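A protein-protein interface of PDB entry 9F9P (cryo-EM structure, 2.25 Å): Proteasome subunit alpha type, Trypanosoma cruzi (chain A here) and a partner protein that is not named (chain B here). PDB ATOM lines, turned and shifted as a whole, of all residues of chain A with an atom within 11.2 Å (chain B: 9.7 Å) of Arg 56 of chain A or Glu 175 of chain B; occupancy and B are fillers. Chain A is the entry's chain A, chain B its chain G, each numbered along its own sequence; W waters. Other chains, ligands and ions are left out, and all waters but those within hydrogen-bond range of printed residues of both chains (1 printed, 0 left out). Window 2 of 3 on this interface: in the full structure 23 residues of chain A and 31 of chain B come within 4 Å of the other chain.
N of Leu 57 of chain A lies close to OD1 of Asp 55 of chain A (3.4 Å).
O of Arg 59 of chain A sits at hydrogen-bond distance from OG1 of Thr 62 of chain A (2.8 Å).
NH1 of Arg 56 of chain A sits at hydrogen-bond distance from O of Glu 175 of chain B, 3.0 Å away.
The backbone NH of Gly 157 of chain B lies within hydrogen-bond range of the side-chain hydroxyl of Thr 62 of chain A (3.2 Å).
N of Tyr 159 of chain B sits at hydrogen-bond distance from O of Leu 57 of chain A (2.9 Å).
The backbone NH (N) of Arg 59 of chain A sits at hydrogen-bond distance from the backbone carbonyl oxygen (O) of Gly 157 of chain B, at 3.0 Å.
OD2 of Asp 55 of chain A touches CE1 of Tyr 158 of chain B (3.9 Å).
Asp 55 of chain A touches Lys 171 of chain B (OD2 to CE, 3.9 Å).
Leu 57 of chain A touches Tyr 158 of chain B.
Leu 57 of chain A touches Gly 160 of chain B.
Phe 179 of chain B touches Leu 57 of chain A.
CA of Met 58 of chain A touches O of Gly 157 of chain B, at 3.7 Å.
Tyr 158 of chain B touches Met 58 of chain A.
Of chain A, only Arg 56 comes within 4 Å of Glu 175 of chain B.
Of chain B, only Tyr 158 and Lys 171 come within 4 Å of Asp 55 of chain A.
No residue of chain A comes within 4 Å of Lys 176 of chain B.
Printed residues of chain B within 4 Å of Met 58 of chain A: Gly 157 (3.7 Å) and Tyr 158 (3.6 Å).
Of the printed residues of chain A, Gly 160 of chain B touches Leu 57.
Ala 37 of chain B touches none of the printed residues of chain A.
Ala 38 of chain B touches none of the printed residues of chain A.
Hydrophobic or aromatic side chains of chain A that line the printed part of chain B: Leu 57 and Met 58.
Of the 25 printed residues of chain B, 7 touch a printed residue of chain A.
Hydrophobic or aromatic side chains of chain B that line the printed part of chain A: Tyr 158, Tyr 159 and Phe 179.
Along chain B the printed residues that touch a printed residue of chain A span positions 157 to 179.
Among the printed residues, 11 pairs touch across the chains.
Among the printed residues, no Asp or Glu carboxylate lies within 4 Å of a Lys or Arg side-chain nitrogen of the other chain.
Water W1 bridges NH2 of Arg 59 of chain A (2.7 Å) and O of Tyr 158 of chain B (2.9 Å).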
ATOM      1  N   ASN A  52       9.853 -12.609   1.057  1.00  0.00           N
ATOM      2  CA  ASN A  52      10.981 -11.737   0.724  1.00  0.00           C
ATOM      3  C   ASN A  52      10.611 -10.261   0.866  1.00  0.00           C
ATOM      4  O   ASN A  52       9.727  -9.715   0.190  1.00  0.00           O
ATOM      5  CB  ASN A  52      11.662 -12.048  -0.612  1.00  0.00           C
ATOM      6  CG  ASN A  52      12.921 -12.872  -0.414  1.00  0.00           C
ATOM      7  OD1 ASN A  52      13.224 -13.309   0.700  1.00  0.00           O
ATOM      8  ND2 ASN A  52      13.653 -13.101  -1.493  1.00  0.00           N
ATOM      9  N   VAL A  53      11.336  -9.656   1.810  1.00  0.00           N
ATOM     10  CA  VAL A  53      11.302  -8.235   2.056  1.00  0.00           C
ATOM     11  C   VAL A  53      12.743  -7.754   1.911  1.00  0.00           C
ATOM     12  O   VAL A  53      13.488  -7.667   2.889  1.00  0.00           O
ATOM     13  CB  VAL A  53      10.681  -7.940   3.434  1.00  0.00           C
ATOM     14  CG1 VAL A  53      10.383  -6.466   3.612  1.00  0.00           C
ATOM     15  CG2 VAL A  53       9.412  -8.752   3.652  1.00  0.00           C
ATOM     16  N   PRO A  54      13.184  -7.480   0.660  1.00  0.00           N
ATOM     17  CA  PRO A  54      14.555  -7.027   0.409  1.00  0.00           C
ATOM     18  C   PRO A  54      14.821  -5.657   1.040  1.00  0.00           C
ATOM     19  O   PRO A  54      15.758  -5.506   1.822  1.00  0.00           O
ATOM     20  CB  PRO A  54      14.659  -6.984  -1.130  1.00  0.00           C
ATOM     21  CG  PRO A  54      13.221  -6.924  -1.642  1.00  0.00           C
ATOM     22  CD  PRO A  54      12.368  -7.560  -0.567  1.00  0.00           C
ATOM     23  N   ASP A  55      13.938  -4.693   0.718  1.00  0.00           N
ATOM     24  CA  ASP A  55      14.019  -3.300   1.141  1.00  0.00           C
ATOM     25  C   ASP A  55      13.698  -3.168   2.634  1.00  0.00           C
ATOM     26  O   ASP A  55      12.637  -3.579   3.089  1.00  0.00           O
ATOM     27  CB  ASP A  55      13.072  -2.475   0.255  1.00  0.00           C
ATOM     28  CG  ASP A  55      13.245  -0.964   0.308  1.00  0.00           C
ATOM     29  OD1 ASP A  55      14.023  -0.481   1.168  1.00  0.00           O
ATOM     30  OD2 ASP A  55      12.604  -0.276  -0.529  1.00  0.00           O
ATOM     31  N   ARG A  56      14.594  -2.527   3.386  1.00  0.00           N
ATOM     32  CA  ARG A  56      14.510  -2.430   4.841  1.00  0.00           C
ATOM     33  C   ARG A  56      13.379  -1.498   5.295  1.00  0.00           C
ATOM     34  O   ARG A  56      12.941  -1.550   6.441  1.00  0.00           O
ATOM     35  CB  ARG A  56      15.862  -1.913   5.343  1.00  0.00           C
ATOM     36  CG  ARG A  56      16.132  -2.150   6.823  1.00  0.00           C
ATOM     37  CD  ARG A  56      17.493  -1.608   7.248  1.00  0.00           C
ATOM     38  NE  ARG A  56      17.536  -0.155   7.408  1.00  0.00           N
ATOM     39  CZ  ARG A  56      16.918   0.530   8.372  1.00  0.00           C
ATOM     40  NH1 ARG A  56      16.991   1.849   8.400  1.00  0.00           N
ATOM     41  NH2 ARG A  56      16.219  -0.103   9.301  1.00  0.00           N
ATOM     42  N   LEU A  57      12.922  -0.647   4.374  1.00  0.00           N
ATOM     43  CA  LEU A  57      11.873   0.336   4.575  1.00  0.00           C
ATOM     44  C   LEU A  57      10.468  -0.211   4.298  1.00  0.00           C
ATOM     45  O   LEU A  57       9.503   0.475   4.581  1.00  0.00           O
ATOM     46  CB  LEU A  57      12.188   1.484   3.611  1.00  0.00           C
ATOM     47  CG  LEU A  57      12.633   2.847   4.169  1.00  0.00           C
ATOM     48  CD1 LEU A  57      13.288   2.777   5.537  1.00  0.00           C
ATOM     49  CD2 LEU A  57      13.568   3.526   3.159  1.00  0.00           C
ATOM     50  N   MET A  58      10.334  -1.420   3.742  1.00  0.00           N
ATOM     51  CA  MET A  58       9.046  -2.044   3.497  1.00  0.00           C
ATOM     52  C   MET A  58       8.432  -2.558   4.786  1.00  0.00           C
ATOM     53  O   MET A  58       9.126  -3.041   5.649  1.00  0.00           O
ATOM     54  CB  MET A  58       9.175  -3.262   2.589  1.00  0.00           C
ATOM     55  CG  MET A  58       8.883  -3.011   1.129  1.00  0.00           C
ATOM     56  SD  MET A  58       8.916  -4.547   0.111  1.00  0.00           S
ATOM     57  CE  MET A  58       9.332  -3.819  -1.477  1.00  0.00           C
ATOM     58  N   ARG A  59       7.113  -2.576   4.835  1.00  0.00           N
ATOM     59  CA  ARG A  59       6.350  -2.991   6.000  1.00  0.00           C
ATOM     60  C   ARG A  59       5.983  -4.463   5.799  1.00  0.00           C
ATOM     61  O   ARG A  59       5.099  -4.783   5.015  1.00  0.00           O
ATOM     62  CB  ARG A  59       5.180  -2.013   6.086  1.00  0.00           C
ATOM     63  CG  ARG A  59       4.240  -2.161   7.262  1.00  0.00           C
ATOM     64  CD  ARG A  59       3.316  -0.966   7.367  1.00  0.00           C
ATOM     65  NE  ARG A  59       2.309  -1.121   8.412  1.00  0.00           N
ATOM     66  CZ  ARG A  59       1.585  -0.120   8.935  1.00  0.00           C
ATOM     67  NH1 ARG A  59       0.733  -0.362   9.918  1.00  0.00           N
ATOM     68  NH2 ARG A  59       1.726   1.127   8.497  1.00  0.00           N
ATOM     69  N   PRO A  60       6.712  -5.415   6.425  1.00  0.00           N
ATOM     70  CA  PRO A  60       6.594  -6.834   6.086  1.00  0.00           C
ATOM     71  C   PRO A  60       5.205  -7.473   6.105  1.00  0.00           C
ATOM     72  O   PRO A  60       4.933  -8.361   5.299  1.00  0.00           O
ATOM     73  CB  PRO A  60       7.483  -7.557   7.119  1.00  0.00           C
ATOM     74  CG  PRO A  60       7.922  -6.495   8.126  1.00  0.00           C
ATOM     75  CD  PRO A  60       7.759  -5.167   7.429  1.00  0.00           C
ATOM     76  N   ASP A  61       4.303  -7.017   6.973  1.00  0.00           N
ATOM     77  CA  ASP A  61       2.981  -7.636   7.056  1.00  0.00           C
ATOM     78  C   ASP A  61       2.054  -7.255   5.887  1.00  0.00           C
ATOM     79  O   ASP A  61       0.908  -7.691   5.854  1.00  0.00           O
ATOM     80  CB  ASP A  61       2.310  -7.290   8.391  1.00  0.00           C
ATOM     81  CG  ASP A  61       2.109  -5.795   8.593  1.00  0.00           C
ATOM     82  OD1 ASP A  61       0.959  -5.325   8.406  1.00  0.00           O
ATOM     83  OD2 ASP A  61       3.106  -5.110   8.938  1.00  0.00           O
ATOM     84  N   THR A  62       2.513  -6.427   4.942  1.00  0.00           N
ATOM     85  CA  THR A  62       1.739  -6.099   3.753  1.00  0.00           C
ATOM     86  C   THR A  62       2.193  -6.914   2.538  1.00  0.00           C
ATOM     87  O   THR A  62       1.603  -6.785   1.479  1.00  0.00           O
ATOM     88  CB  THR A  62       1.820  -4.600   3.412  1.00  0.00           C
ATOM     89  OG1 THR A  62       3.151  -4.234   3.029  1.00  0.00           O
ATOM     90  CG2 THR A  62       1.389  -3.706   4.551  1.00  0.00           C
ATOM     91  N   ILE A  63       3.253  -7.724   2.666  1.00  0.00           N
ATOM     92  CA  ILE A  63       3.723  -8.524   1.542  1.00  0.00           C
ATOM     93  C   ILE A  63       3.376  -9.988   1.815  1.00  0.00           C
ATOM     94  O   ILE A  63       3.967 -10.601   2.702  1.00  0.00           O
ATOM     95  CB  ILE A  63       5.245  -8.368   1.314  1.00  0.00           C
ATOM     96  CG1 ILE A  63       5.749  -6.929   1.512  1.00  0.00           C
ATOM     97  CG2 ILE A  63       5.646  -8.916  -0.047  1.00  0.00           C
ATOM     98  CD1 ILE A  63       5.072  -5.888   0.633  1.00  0.00           C
ATOM     99  N   ALA B  37       8.085  10.003   0.968  1.00  0.00           N
ATOM    100  CA  ALA B  37       7.010   9.957   1.942  1.00  0.00           C
ATOM    101  C   ALA B  37       7.413   9.155   3.157  1.00  0.00           C
ATOM    102  O   ALA B  37       8.288   8.317   3.071  1.00  0.00           O
ATOM    103  CB  ALA B  37       5.779   9.385   1.298  1.00  0.00           C
ATOM    104  N   ALA B  38       6.753   9.444   4.280  1.00  0.00           N
ATOM    105  CA  ALA B  38       7.071   8.844   5.568  1.00  0.00           C
ATOM    106  C   ALA B  38       5.815   8.663   6.400  1.00  0.00           C
ATOM    107  O   ALA B  38       4.930   9.499   6.371  1.00  0.00           O
ATOM    108  CB  ALA B  38       8.030   9.745   6.281  1.00  0.00           C
ATOM    109  N   GLY B 157       3.259  -1.911   0.885  1.00  0.00           N
ATOM    110  CA  GLY B 157       3.230  -1.003   2.015  1.00  0.00           C
ATOM    111  C   GLY B 157       4.618  -0.648   2.539  1.00  0.00           C
ATOM    112  O   GLY B 157       5.500  -1.498   2.607  1.00  0.00           O
ATOM    113  N   TYR B 158       4.802   0.602   2.942  1.00  0.00           N
ATOM    114  CA  TYR B 158       6.118   1.083   3.342  1.00  0.00           C
ATOM    115  C   TYR B 158       6.048   1.913   4.603  1.00  0.00           C
ATOM    116  O   TYR B 158       5.005   2.459   4.909  1.00  0.00           O
ATOM    117  CB  TYR B 158       6.715   1.969   2.253  1.00  0.00           C
ATOM    118  CG  TYR B 158       7.081   1.252   0.974  1.00  0.00           C
ATOM    119  CD1 TYR B 158       8.387   0.871   0.716  1.00  0.00           C
ATOM    120  CD2 TYR B 158       6.136   1.012  -0.012  1.00  0.00           C
ATOM    121  CE1 TYR B 158       8.742   0.256  -0.470  1.00  0.00           C
ATOM    122  CE2 TYR B 158       6.469   0.383  -1.204  1.00  0.00           C
ATOM    123  CZ  TYR B 158       7.775  -0.019  -1.427  1.00  0.00           C
ATOM    124  OH  TYR B 158       8.128  -0.634  -2.612  1.00  0.00           O
ATOM    125  N   TYR B 159       7.180   2.042   5.300  1.00  0.00           N
ATOM    126  CA  TYR B 159       7.365   3.046   6.350  1.00  0.00           C
ATOM    127  C   TYR B 159       7.882   4.356   5.775  1.00  0.00           C
ATOM    128  O   TYR B 159       7.624   5.399   6.337  1.00  0.00           O
ATOM    129  CB  TYR B 159       8.377   2.608   7.414  1.00  0.00           C
ATOM    130  CG  TYR B 159       7.968   1.414   8.256  1.00  0.00           C
ATOM    131  CD1 TYR B 159       6.817   1.434   9.030  1.00  0.00           C
ATOM    132  CD2 TYR B 159       8.717   0.237   8.246  1.00  0.00           C
ATOM    133  CE1 TYR B 159       6.418   0.320   9.764  1.00  0.00           C
ATOM    134  CE2 TYR B 159       8.352  -0.871   8.991  1.00  0.00           C
ATOM    135  CZ  TYR B 159       7.207  -0.819   9.765  1.00  0.00           C
ATOM    136  OH  TYR B 159       6.847  -1.923  10.495  1.00  0.00           O
ATOM    137  N   GLY B 160       8.707   4.283   4.737  1.00  0.00           N
ATOM    138  CA  GLY B 160       9.229   5.440   4.040  1.00  0.00           C
ATOM    139  C   GLY B 160       9.576   5.035   2.615  1.00  0.00           C
ATOM    140  O   GLY B 160       9.813   3.852   2.391  1.00  0.00           O
ATOM    141  N   ILE B 161       9.522   5.956   1.648  1.00  0.00           N
ATOM    142  CA  ILE B 161       9.713   5.564   0.259  1.00  0.00           C
ATOM    143  C   ILE B 161      10.169   6.759  -0.545  1.00  0.00           C
ATOM    144  O   ILE B 161       9.910   7.872  -0.153  1.00  0.00           O
ATOM    145  CB  ILE B 161       8.463   4.917  -0.384  1.00  0.00           C
ATOM    146  CG1 ILE B 161       8.746   4.268  -1.752  1.00  0.00           C
ATOM    147  CG2 ILE B 161       7.329   5.897  -0.535  1.00  0.00           C
ATOM    148  CD1 ILE B 161       9.921   3.243  -1.757  1.00  0.00           C
ATOM    149  N   ALA B 162      10.920   6.494  -1.618  1.00  0.00           N
ATOM    150  CA  ALA B 162      11.290   7.491  -2.610  1.00  0.00           C
ATOM    151  C   ALA B 162      11.124   6.942  -4.015  1.00  0.00           C
ATOM    152  O   ALA B 162      11.438   5.790  -4.262  1.00  0.00           O
ATOM    153  CB  ALA B 162      12.720   7.904  -2.408  1.00  0.00           C
ATOM    154  N   LYS B 167      15.934   8.776  -6.529  1.00  0.00           N
ATOM    155  CA  LYS B 167      15.492   7.825  -5.523  1.00  0.00           C
ATOM    156  C   LYS B 167      16.633   7.081  -4.849  1.00  0.00           C
ATOM    157  O   LYS B 167      16.490   6.749  -3.682  1.00  0.00           O
ATOM    158  CB  LYS B 167      14.493   6.793  -6.050  1.00  0.00           C
ATOM    159  CG  LYS B 167      14.968   5.888  -7.165  1.00  0.00           C
ATOM    160  CD  LYS B 167      14.095   4.669  -7.354  1.00  0.00           C
ATOM    161  CE  LYS B 167      14.428   3.985  -8.663  1.00  0.00           C
ATOM    162  NZ  LYS B 167      14.119   2.539  -8.615  1.00  0.00           N
ATOM    163  N   THR B 168      17.735   6.793  -5.534  1.00  0.00           N
ATOM    164  CA  THR B 168      18.792   5.982  -4.931  1.00  0.00           C
ATOM    165  C   THR B 168      19.414   6.711  -3.729  1.00  0.00           C
ATOM    166  O   THR B 168      19.514   6.141  -2.642  1.00  0.00           O
ATOM    167  CB  THR B 168      19.806   5.536  -5.998  1.00  0.00           C
ATOM    168  OG1 THR B 168      19.213   4.469  -6.741  1.00  0.00           O
ATOM    169  CG2 THR B 168      21.114   5.052  -5.419  1.00  0.00           C
ATOM    170  N   VAL B 169      19.768   7.990  -3.914  1.00  0.00           N
ATOM    171  CA  VAL B 169      20.297   8.826  -2.847  1.00  0.00           C
ATOM    172  C   VAL B 169      19.240   9.101  -1.770  1.00  0.00           C
ATOM    173  O   VAL B 169      19.520   9.035  -0.578  1.00  0.00           O
ATOM    174  CB  VAL B 169      20.839  10.148  -3.420  1.00  0.00           C
ATOM    175  CG1 VAL B 169      21.257  11.104  -2.311  1.00  0.00           C
ATOM    176  CG2 VAL B 169      21.979   9.906  -4.400  1.00  0.00           C
ATOM    177  N   ALA B 170      18.018   9.439  -2.180  1.00  0.00           N
ATOM    178  CA  ALA B 170      16.982   9.791  -1.226  1.00  0.00           C
ATOM    179  C   ALA B 170      16.718   8.641  -0.248  1.00  0.00           C
ATOM    180  O   ALA B 170      16.486   8.897   0.931  1.00  0.00           O
ATOM    181  CB  ALA B 170      15.733  10.210  -1.972  1.00  0.00           C
ATOM    182  N   LYS B 171      16.760   7.391  -0.735  1.00  0.00           N
ATOM    183  CA  LYS B 171      16.553   6.177   0.060  1.00  0.00           C
ATOM    184  C   LYS B 171      17.583   6.070   1.184  1.00  0.00           C
ATOM    185  O   LYS B 171      17.242   5.731   2.316  1.00  0.00           O
ATOM    186  CB  LYS B 171      16.795   4.920  -0.781  1.00  0.00           C
ATOM    187  CG  LYS B 171      15.720   3.847  -0.731  1.00  0.00           C
ATOM    188  CD  LYS B 171      14.724   3.993  -1.869  1.00  0.00           C
ATOM    189  CE  LYS B 171      14.302   2.672  -2.477  1.00  0.00           C
ATOM    190  NZ  LYS B 171      13.976   2.841  -3.912  1.00  0.00           N
ATOM    191  N   THR B 172      18.850   6.339   0.838  1.00  0.00           N
ATOM    192  CA  THR B 172      19.947   6.392   1.795  1.00  0.00           C
ATOM    193  C   THR B 172      19.616   7.290   2.991  1.00  0.00           C
ATOM    194  O   THR B 172      19.907   6.930   4.126  1.00  0.00           O
ATOM    195  CB  THR B 172      21.226   6.890   1.105  1.00  0.00           C
ATOM    196  OG1 THR B 172      21.516   6.015   0.018  1.00  0.00           O
ATOM    197  CG2 THR B 172      22.418   6.962   2.034  1.00  0.00           C
ATOM    198  N   GLU B 173      19.027   8.461   2.738  1.00  0.00           N
ATOM    199  CA  GLU B 173      18.743   9.452   3.766  1.00  0.00           C
ATOM    200  C   GLU B 173      17.480   9.126   4.579  1.00  0.00           C
ATOM    201  O   GLU B 173      17.349   9.600   5.703  1.00  0.00           O
ATOM    202  CB  GLU B 173      18.567  10.824   3.113  1.00  0.00           C
ATOM    203  CG  GLU B 173      19.792  11.349   2.379  1.00  0.00           C
ATOM    204  CD  GLU B 173      20.968  11.702   3.280  1.00  0.00           C
ATOM    205  OE1 GLU B 173      22.101  11.266   2.960  1.00  0.00           O
ATOM    206  OE2 GLU B 173      20.744  12.392   4.317  1.00  0.00           O
ATOM    207  N   LEU B 174      16.515   8.394   3.998  1.00  0.00           N
ATOM    208  CA  LEU B 174      15.323   7.957   4.716  1.00  0.00           C
ATOM    209  C   LEU B 174      15.667   6.820   5.678  1.00  0.00           C
ATOM    210  O   LEU B 174      14.853   6.493   6.540  1.00  0.00           O
ATOM    211  CB  LEU B 174      14.252   7.439   3.744  1.00  0.00           C
ATOM    212  CG  LEU B 174      13.503   8.460   2.891  1.00  0.00           C
ATOM    213  CD1 LEU B 174      12.703   7.762   1.814  1.00  0.00           C
ATOM    214  CD2 LEU B 174      12.575   9.307   3.729  1.00  0.00           C
ATOM    215  N   GLU B 175      16.810   6.157   5.477  1.00  0.00           N
ATOM    216  CA  GLU B 175      17.192   5.033   6.316  1.00  0.00           C
ATOM    217  C   GLU B 175      17.791   5.528   7.637  1.00  0.00           C
ATOM    218  O   GLU B 175      17.868   4.751   8.589  1.00  0.00           O
ATOM    219  CB  GLU B 175      18.123   4.092   5.547  1.00  0.00           C
ATOM    220  CG  GLU B 175      17.362   3.145   4.622  1.00  0.00           C
ATOM    221  CD  GLU B 175      18.167   2.350   3.594  1.00  0.00           C
ATOM    222  OE1 GLU B 175      18.026   1.107   3.566  1.00  0.00           O
ATOM    223  OE2 GLU B 175      18.911   2.970   2.802  1.00  0.00           O
ATOM    224  N   LYS B 176      18.170   6.820   7.710  1.00  0.00           N
ATOM    225  CA  LYS B 176      18.669   7.437   8.938  1.00  0.00           C
ATOM    226  C   LYS B 176      17.571   8.195   9.687  1.00  0.00           C
ATOM    227  O   LYS B 176      17.864   9.193  10.347  1.00  0.00           O
ATOM    228  CB  LYS B 176      19.739   8.487   8.637  1.00  0.00           C
ATOM    229  CG  LYS B 176      20.828   8.085   7.657  1.00  0.00           C
ATOM    230  CD  LYS B 176      21.862   9.180   7.488  1.00  0.00           C
ATOM    231  CE  LYS B 176      23.076   8.755   6.686  1.00  0.00           C
ATOM    232  NZ  LYS B 176      22.946   9.136   5.258  1.00  0.00           N
ATOM    233  N   LEU B 177      16.304   7.790   9.527  1.00  0.00           N
ATOM    234  CA  LEU B 177      15.214   8.330  10.329  1.00  0.00           C
ATOM    235  C   LEU B 177      14.709   7.244  11.270  1.00  0.00           C
ATOM    236  O   LEU B 177      14.840   6.053  10.985  1.00  0.00           O
ATOM    237  CB  LEU B 177      14.045   8.801   9.450  1.00  0.00           C
ATOM    238  CG  LEU B 177      14.318   9.875   8.393  1.00  0.00           C
ATOM    239  CD1 LEU B 177      13.004  10.482   7.911  1.00  0.00           C
ATOM    240  CD2 LEU B 177      15.252  10.965   8.899  1.00  0.00           C
ATOM    241  N   ASN B 178      14.074   7.681  12.356  1.00  0.00           N
ATOM    242  CA  ASN B 178      13.479   6.783  13.329  1.00  0.00           C
ATOM    243  C   ASN B 178      11.959   6.899  13.209  1.00  0.00           C
ATOM    244  O   ASN B 178      11.388   7.931  13.544  1.00  0.00           O
ATOM    245  CB  ASN B 178      14.013   7.096  14.731  1.00  0.00           C
ATOM    246  CG  ASN B 178      13.398   6.242  15.820  1.00  0.00           C
ATOM    247  OD1 ASN B 178      12.883   5.155  15.563  1.00  0.00           O
ATOM    248  ND2 ASN B 178      13.455   6.726  17.049  1.00  0.00           N
ATOM    249  N   PHE B 179      11.312   5.822  12.742  1.00  0.00           N
ATOM    250  CA  PHE B 179       9.935   5.890  12.263  1.00  0.00           C
ATOM    251  C   PHE B 179       8.928   5.767  13.410  1.00  0.00           C
ATOM    252  O   PHE B 179       7.815   6.292  13.306  1.00  0.00           O
ATOM    253  CB  PHE B 179       9.716   4.856  11.150  1.00  0.00           C
ATOM    254  CG  PHE B 179      10.314   5.295   9.839  1.00  0.00           C
ATOM    255  CD1 PHE B 179       9.802   6.391   9.166  1.00  0.00           C
ATOM    256  CD2 PHE B 179      11.439   4.679   9.327  1.00  0.00           C
ATOM    257  CE1 PHE B 179      10.382   6.840   7.991  1.00  0.00           C
ATOM    258  CE2 PHE B 179      12.027   5.134   8.159  1.00  0.00           C
ATOM    259  CZ  PHE B 179      11.497   6.210   7.488  1.00  0.00           C
ATOM    260  N   LYS B 180       9.332   5.103  14.500  1.00  0.00           N
ATOM    261  CA  LYS B 180       8.478   4.922  15.666  1.00  0.00           C
ATOM    262  C   LYS B 180       8.291   6.227  16.451  1.00  0.00           C
ATOM    263  O   LYS B 180       7.275   6.380  17.124  1.00  0.00           O
ATOM    264  CB  LYS B 180       9.063   3.818  16.551  1.00  0.00           C
ATOM    265  CG  LYS B 180       9.114   2.451  15.885  1.00  0.00           C
ATOM    266  CD  LYS B 180       9.914   1.412  16.637  1.00  0.00           C
ATOM    267  CE  LYS B 180       9.952   0.086  15.908  1.00  0.00           C
ATOM    268  NZ  LYS B 180      10.809  -0.902  16.606  1.00  0.00           N
ATOM    269  N   LYS B 190      12.607  17.383   7.533  1.00  0.00           N
ATOM    270  CA  LYS B 190      13.558  16.397   7.039  1.00  0.00           C
ATOM    271  C   LYS B 190      13.302  16.027   5.580  1.00  0.00           C
ATOM    272  O   LYS B 190      14.240  15.861   4.798  1.00  0.00           O
ATOM    273  CB  LYS B 190      13.506  15.124   7.880  1.00  0.00           C
ATOM    274  CG  LYS B 190      13.741  15.394   9.361  1.00  0.00           C
ATOM    275  CD  LYS B 190      14.899  14.627   9.965  1.00  0.00           C
ATOM    276  CE  LYS B 190      14.793  14.525  11.471  1.00  0.00           C
ATOM    277  NZ  LYS B 190      15.880  13.686  12.034  1.00  0.00           N
ATOM    278  N   LEU B 191      12.029  15.829   5.246  1.00  0.00           N
ATOM    279  CA  LEU B 191      11.668  15.404   3.912  1.00  0.00           C
ATOM    280  C   LEU B 191      11.987  16.524   2.926  1.00  0.00           C
ATOM    281  O   LEU B 191      12.470  16.248   1.824  1.00  0.00           O
ATOM    282  CB  LEU B 191      10.182  15.052   3.897  1.00  0.00           C
ATOM    283  CG  LEU B 191       9.809  13.573   3.870  1.00  0.00           C
ATOM    284  CD1 LEU B 191      10.592  12.711   4.856  1.00  0.00           C
ATOM    285  CD2 LEU B 191       8.325  13.459   4.138  1.00  0.00           C
ATOM    286  N   ILE B 194      15.766  16.577   2.123  1.00  0.00           N
ATOM    287  CA  ILE B 194      16.218  15.541   1.207  1.00  0.00           C
ATOM    288  C   ILE B 194      15.962  15.970  -0.238  1.00  0.00           C
ATOM    289  O   ILE B 194      16.834  15.824  -1.093  1.00  0.00           O
ATOM    290  CB  ILE B 194      15.573  14.196   1.581  1.00  0.00           C
ATOM    291  CG1 ILE B 194      16.078  13.703   2.942  1.00  0.00           C
ATOM    292  CG2 ILE B 194      15.810  13.150   0.516  1.00  0.00           C
ATOM    293  CD1 ILE B 194      15.190  12.650   3.594  1.00  0.00           C
HETATM  294  O   HOH W   1       2.411   1.984   5.998  1.00  0.00           O
